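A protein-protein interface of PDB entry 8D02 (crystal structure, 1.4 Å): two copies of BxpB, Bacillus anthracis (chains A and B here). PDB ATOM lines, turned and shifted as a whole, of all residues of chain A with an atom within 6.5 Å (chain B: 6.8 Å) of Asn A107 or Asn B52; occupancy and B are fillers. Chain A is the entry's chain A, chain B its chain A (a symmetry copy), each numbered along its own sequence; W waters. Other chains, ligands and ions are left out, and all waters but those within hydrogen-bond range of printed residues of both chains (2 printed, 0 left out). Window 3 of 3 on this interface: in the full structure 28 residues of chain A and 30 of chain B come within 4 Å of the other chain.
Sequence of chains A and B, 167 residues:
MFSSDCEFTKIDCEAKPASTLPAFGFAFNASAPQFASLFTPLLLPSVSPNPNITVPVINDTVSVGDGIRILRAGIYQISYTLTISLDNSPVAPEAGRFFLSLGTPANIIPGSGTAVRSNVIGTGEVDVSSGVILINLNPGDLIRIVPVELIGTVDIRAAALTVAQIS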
ATOM      1  N   PHE A  39     -23.390  -5.743 -14.195  1.00  0.00           N
ATOM      2  CA  PHE A  39     -23.567  -5.197 -15.535  1.00  0.00           C
ATOM      3  C   PHE A  39     -23.176  -3.742 -15.631  1.00  0.00           C
ATOM      4  O   PHE A  39     -23.669  -2.987 -16.470  1.00  0.00           O
ATOM      5  CB  PHE A  39     -24.945  -5.539 -16.127  1.00  0.00           C
ATOM      6  CG  PHE A  39     -25.144  -7.005 -16.256  1.00  0.00           C
ATOM      7  CD1 PHE A  39     -24.519  -7.674 -17.301  1.00  0.00           C
ATOM      8  CD2 PHE A  39     -25.873  -7.731 -15.331  1.00  0.00           C
ATOM      9  CE1 PHE A  39     -24.625  -9.017 -17.449  1.00  0.00           C
ATOM     10  CE2 PHE A  39     -25.988  -9.114 -15.475  1.00  0.00           C
ATOM     11  CZ  PHE A  39     -25.340  -9.741 -16.544  1.00  0.00           C
ATOM     12  N   LEU A 100     -15.297  -9.542 -20.826  1.00  0.00           N
ATOM     13  CA  LEU A 100     -15.356  -8.403 -21.721  1.00  0.00           C
ATOM     14  C   LEU A 100     -16.713  -8.405 -22.413  1.00  0.00           C
ATOM     15  O   LEU A 100     -17.272  -9.460 -22.701  1.00  0.00           O
ATOM     16  CB  LEU A 100     -14.250  -8.570 -22.751  1.00  0.00           C
ATOM     17  CG  LEU A 100     -12.842  -8.480 -22.210  1.00  0.00           C
ATOM     18  CD1 LEU A 100     -11.827  -8.910 -23.272  1.00  0.00           C
ATOM     19  CD2 LEU A 100     -12.573  -7.061 -21.721  1.00  0.00           C
ATOM     20  N   SER A 101     -17.234  -7.207 -22.657  1.00  0.00           N
ATOM     21  CA  SER A 101     -18.508  -6.982 -23.327  1.00  0.00           C
ATOM     22  C   SER A 101     -18.295  -6.185 -24.605  1.00  0.00           C
ATOM     23  O   SER A 101     -17.366  -5.362 -24.697  1.00  0.00           O
ATOM     24  CB  SER A 101     -19.518  -6.273 -22.402  1.00  0.00           C
ATOM     25  OG  SER A 101     -19.119  -4.937 -22.147  1.00  0.00           O
ATOM     26  N   LEU A 102     -19.164  -6.440 -25.571  1.00  0.00           N
ATOM     27  CA  LEU A 102     -19.171  -5.765 -26.855  1.00  0.00           C
ATOM     28  C   LEU A 102     -20.461  -4.954 -26.969  1.00  0.00           C
ATOM     29  O   LEU A 102     -21.551  -5.520 -27.118  1.00  0.00           O
ATOM     30  CB  LEU A 102     -19.096  -6.861 -27.933  1.00  0.00           C
ATOM     31  CG  LEU A 102     -19.054  -6.404 -29.382  1.00  0.00           C
ATOM     32  CD1 LEU A 102     -17.925  -5.537 -29.646  1.00  0.00           C
ATOM     33  CD2 LEU A 102     -19.052  -7.584 -30.368  1.00  0.00           C
ATOM     34  N   GLY A 103     -20.345  -3.642 -26.909  1.00  0.00           N
ATOM     35  CA  GLY A 103     -21.564  -2.832 -26.958  1.00  0.00           C
ATOM     36  C   GLY A 103     -22.276  -2.792 -25.604  1.00  0.00           C
ATOM     37  O   GLY A 103     -21.700  -2.373 -24.578  1.00  0.00           O
ATOM     38  N   THR A 104     -23.523  -3.226 -25.545  1.00  0.00           N
ATOM     39  CA  THR A 104     -24.253  -3.166 -24.286  1.00  0.00           C
ATOM     40  C   THR A 104     -23.603  -4.111 -23.263  1.00  0.00           C
ATOM     41  O   THR A 104     -23.085  -5.175 -23.633  1.00  0.00           O
ATOM     42  CB  THR A 104     -25.735  -3.473 -24.554  1.00  0.00           C
ATOM     43  OG1 THR A 104     -26.522  -3.046 -23.427  1.00  0.00           O
ATOM     44  CG2 THR A 104     -25.931  -4.907 -24.828  1.00  0.00           C
ATOM     45  N   PRO A 105     -23.627  -3.765 -21.965  1.00  0.00           N
ATOM     46  CA  PRO A 105     -22.877  -4.570 -20.990  1.00  0.00           C
ATOM     47  C   PRO A 105     -23.268  -6.022 -20.925  1.00  0.00           C
ATOM     48  O   PRO A 105     -22.406  -6.848 -20.603  1.00  0.00           O
ATOM     49  CB  PRO A 105     -23.127  -3.840 -19.662  1.00  0.00           C
ATOM     50  CG  PRO A 105     -23.344  -2.437 -20.077  1.00  0.00           C
ATOM     51  CD  PRO A 105     -24.092  -2.499 -21.391  1.00  0.00           C
ATOM     52  N   ALA A 106     -24.521  -6.390 -21.198  1.00  0.00           N
ATOM     53  CA  ALA A 106     -24.914  -7.800 -21.160  1.00  0.00           C
ATOM     54  C   ALA A 106     -24.435  -8.611 -22.347  1.00  0.00           C
ATOM     55  O   ALA A 106     -24.522  -9.841 -22.279  1.00  0.00           O
ATOM     56  CB  ALA A 106     -26.429  -7.952 -21.058  1.00  0.00           C
ATOM     57  N   ASN A 107     -23.906  -7.956 -23.391  1.00  0.00           N
ATOM     58  CA  ASN A 107     -23.437  -8.620 -24.604  1.00  0.00           C
ATOM     59  C   ASN A 107     -22.008  -9.131 -24.398  1.00  0.00           C
ATOM     60  O   ASN A 107     -21.049  -8.674 -25.023  1.00  0.00           O
ATOM     61  CB  ASN A 107     -23.567  -7.676 -25.799  1.00  0.00           C
ATOM     62  CG  ASN A 107     -23.568  -8.383 -27.115  1.00  0.00           C
ATOM     63  OD1 ASN A 107     -23.966  -9.563 -27.210  1.00  0.00           O
ATOM     64  ND2 ASN A 107     -23.055  -7.710 -28.124  1.00  0.00           N
ATOM     65  N   ILE A 108     -21.893 -10.153 -23.551  1.00  0.00           N
ATOM     66  CA  ILE A 108     -20.577 -10.635 -23.145  1.00  0.00           C
ATOM     67  C   ILE A 108     -19.907 -11.429 -24.258  1.00  0.00           C
ATOM     68  O   ILE A 108     -20.554 -12.017 -25.141  1.00  0.00           O
ATOM     69  CB  ILE A 108     -20.654 -11.435 -21.845  1.00  0.00           C
ATOM     70  CG1 ILE A 108     -21.556 -12.676 -21.977  1.00  0.00           C
ATOM     71  CG2 ILE A 108     -21.135 -10.509 -20.743  1.00  0.00           C
ATOM     72  CD1 ILE A 108     -21.479 -13.581 -20.743  1.00  0.00           C
ATOM     73  N   ILE A 109     -18.577 -11.505 -24.175  1.00  0.00           N
ATOM     74  CA  ILE A 109     -17.742 -12.204 -25.155  1.00  0.00           C
ATOM     75  C   ILE A 109     -17.348 -13.567 -24.584  1.00  0.00           C
ATOM     76  O   ILE A 109     -16.485 -13.621 -23.688  1.00  0.00           O
ATOM     77  CB  ILE A 109     -16.523 -11.358 -25.522  1.00  0.00           C
ATOM     78  CG1 ILE A 109     -17.008 -10.082 -26.222  1.00  0.00           C
ATOM     79  CG2 ILE A 109     -15.583 -12.109 -26.439  1.00  0.00           C
ATOM     80  CD1 ILE A 109     -15.964  -8.963 -26.294  1.00  0.00           C
ATOM     81  N   ASP A 141     -17.480  -0.670 -32.346  1.00  0.00           N
ATOM     82  CA  ASP A 141     -17.531  -1.635 -31.246  1.00  0.00           C
ATOM     83  C   ASP A 141     -16.903  -1.072 -29.968  1.00  0.00           C
ATOM     84  O   ASP A 141     -15.763  -0.604 -29.974  1.00  0.00           O
ATOM     85  CB  ASP A 141     -16.755  -2.889 -31.668  1.00  0.00           C
ATOM     86  CG  ASP A 141     -17.543  -3.775 -32.639  1.00  0.00           C
ATOM     87  OD1 ASP A 141     -18.754  -3.594 -32.870  1.00  0.00           O
ATOM     88  OD2 ASP A 141     -16.926  -4.719 -33.144  1.00  0.00           O
ATOM     89  N   PRO B  49     -15.470 -16.169 -30.646  1.00  0.00           N
ATOM     90  CA  PRO B  49     -15.857 -15.382 -29.461  1.00  0.00           C
ATOM     91  C   PRO B  49     -16.773 -14.200 -29.701  1.00  0.00           C
ATOM     92  O   PRO B  49     -17.449 -13.787 -28.742  1.00  0.00           O
ATOM     93  CB  PRO B  49     -14.506 -14.851 -28.960  1.00  0.00           C
ATOM     94  CG  PRO B  49     -13.691 -14.703 -30.198  1.00  0.00           C
ATOM     95  CD  PRO B  49     -14.090 -15.885 -31.079  1.00  0.00           C
ATOM     96  N   ASN B  50     -16.836 -13.615 -30.886  1.00  0.00           N
ATOM     97  CA  ASN B  50     -17.620 -12.388 -31.070  1.00  0.00           C
ATOM     98  C   ASN B  50     -19.099 -12.749 -31.041  1.00  0.00           C
ATOM     99  O   ASN B  50     -19.536 -13.559 -31.874  1.00  0.00           O
ATOM    100  CB  ASN B  50     -17.239 -11.737 -32.404  1.00  0.00           C
ATOM    101  CG  ASN B  50     -17.904 -10.390 -32.630  1.00  0.00           C
ATOM    102  OD1 ASN B  50     -19.098 -10.257 -32.397  1.00  0.00           O
ATOM    103  ND2 ASN B  50     -17.177  -9.432 -33.121  1.00  0.00           N
ATOM    104  N   PRO B  51     -19.910 -12.184 -30.142  1.00  0.00           N
ATOM    105  CA  PRO B  51     -21.341 -12.541 -30.053  1.00  0.00           C
ATOM    106  C   PRO B  51     -22.210 -11.925 -31.136  1.00  0.00           C
ATOM    107  O   PRO B  51     -23.369 -12.363 -31.272  1.00  0.00           O
ATOM    108  CB  PRO B  51     -21.762 -11.965 -28.689  1.00  0.00           C
ATOM    109  CG  PRO B  51     -20.729 -10.967 -28.328  1.00  0.00           C
ATOM    110  CD  PRO B  51     -19.528 -11.125 -29.178  1.00  0.00           C
ATOM    111  N   ASN B  52     -21.720 -10.930 -31.865  1.00  0.00           N
ATOM    112  CA  ASN B  52     -22.461 -10.279 -32.954  1.00  0.00           C
ATOM    113  C   ASN B  52     -22.162 -10.868 -34.321  1.00  0.00           C
ATOM    114  O   ASN B  52     -23.084 -11.113 -35.104  1.00  0.00           O
ATOM    115  CB  ASN B  52     -22.158  -8.792 -32.996  1.00  0.00           C
ATOM    116  CG  ASN B  52     -22.649  -8.052 -31.776  1.00  0.00           C
ATOM    117  OD1 ASN B  52     -23.360  -8.600 -30.943  1.00  0.00           O
ATOM    118  ND2 ASN B  52     -22.315  -6.791 -31.699  1.00  0.00           N
ATOM    119  N   ILE B  53     -20.896 -11.090 -34.616  1.00  0.00           N
ATOM    120  CA  ILE B  53     -20.407 -11.573 -35.907  1.00  0.00           C
ATOM    121  C   ILE B  53     -19.551 -12.766 -35.520  1.00  0.00           C
ATOM    122  O   ILE B  53     -18.343 -12.620 -35.283  1.00  0.00           O
ATOM    123  CB  ILE B  53     -19.601 -10.506 -36.647  1.00  0.00           C
ATOM    124  CG1 ILE B  53     -20.432  -9.214 -36.779  1.00  0.00           C
ATOM    125  CG2 ILE B  53     -19.006 -11.043 -37.965  1.00  0.00           C
ATOM    126  CD1 ILE B  53     -19.850  -8.186 -37.737  1.00  0.00           C
ATOM    127  N   THR B  54     -20.186 -13.930 -35.369  1.00  0.00           N
ATOM    128  CA  THR B  54     -19.650 -15.060 -34.611  1.00  0.00           C
ATOM    129  C   THR B  54     -18.900 -16.005 -35.533  1.00  0.00           C
ATOM    130  O   THR B  54     -19.488 -16.938 -36.091  1.00  0.00           O
ATOM    131  CB  THR B  54     -20.772 -15.766 -33.860  1.00  0.00           C
ATOM    132  OG1 THR B  54     -21.536 -14.785 -33.129  1.00  0.00           O
ATOM    133  CG2 THR B  54     -20.220 -16.813 -32.909  1.00  0.00           C
HETATM  134  O   HOH W   1     -20.349  -5.734 -33.775  1.00  0.00           O
HETATM  135  O   HOH W   2     -17.939  -6.880 -34.327  1.00  0.00           O
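The side-chain amide nitrogen (ND2) of Asn A107 is in hydrogen-bond range of the side-chain amide oxygen (OD1) of Asn B52 (3.0 Å).
The side-chain hydroxyl (OG1) of Thr B54 lies within hydrogen-bond range of the backbone carbonyl oxygen (O) of Asn B50 (2.7 Å).
The side-chain amide oxygen of Asn B50 is in hydrogen-bond range of the backbone NH of Ile B53, at 3.0 Å.
The backbone carbonyl oxygen (O) of Leu A100 lies within hydrogen-bond range of the backbone NH (N) of Ile A109 (2.8 Å).
OD1 of Asn B50 lies within hydrogen-bond range of N of Asn B52, 2.8 Å away.
The side-chain amide nitrogen of Asn A107 is in hydrogen-bond range of the backbone carbonyl oxygen of Leu A102, at 2.8 Å.
CD2 of Leu A102 touches OD1 of Asn B50 (3.4 Å).
CD of Pro B51 touches CD2 of Leu A102 (3.8 Å).
CD2 of Leu A102 touches ND2 of Asn B52 (3.6 Å).
Pro B51 touches Asn A107 (CB to OD1, 3.6 Å).
CG of Pro B51 touches O of Ile A108, at 3.4 Å.
Pro B49 touches Ile A109 (O to CG2, 3.4 Å).
Asn A107 touches just these residues of chain B: Pro B51 (3.6 Å) and Asn B52 (3.0 Å).
Asn B52 touches just these residues of chain A: Leu A102 (3.6 Å) and Asn A107 (3.0 Å).
Printed residues of chain B within 4 Å of Leu A102: Asn B50 (3.4 Å), Pro B51 (3.8 Å) and Asn B52 (3.6 Å).
Printed residues of chain A within 4 Å of Pro B49: Ile A109 (3.4 Å).
Pro A105 touches none of the printed residues of chain B.
The nearest residue of chain A that does not touch Asn B52 is Asp A141 (4.9 Å).
Of the 12 printed residues of chain A, 4 touch a printed residue of chain B.
Printed residues of chain A that touch a printed residue of chain B: Leu A102, Asn A107, Ile A108 and Ile A109.
No position is printed for both chains.
Water W2 lies within hydrogen-bond range of the side-chain carboxylate of Asp A141 and the side-chain amide nitrogen of Asn B50.
Water W1 lies within hydrogen-bond range of the side-chain carboxylate of Asp A141 and the side-chain amide nitrogen of Asn B52.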
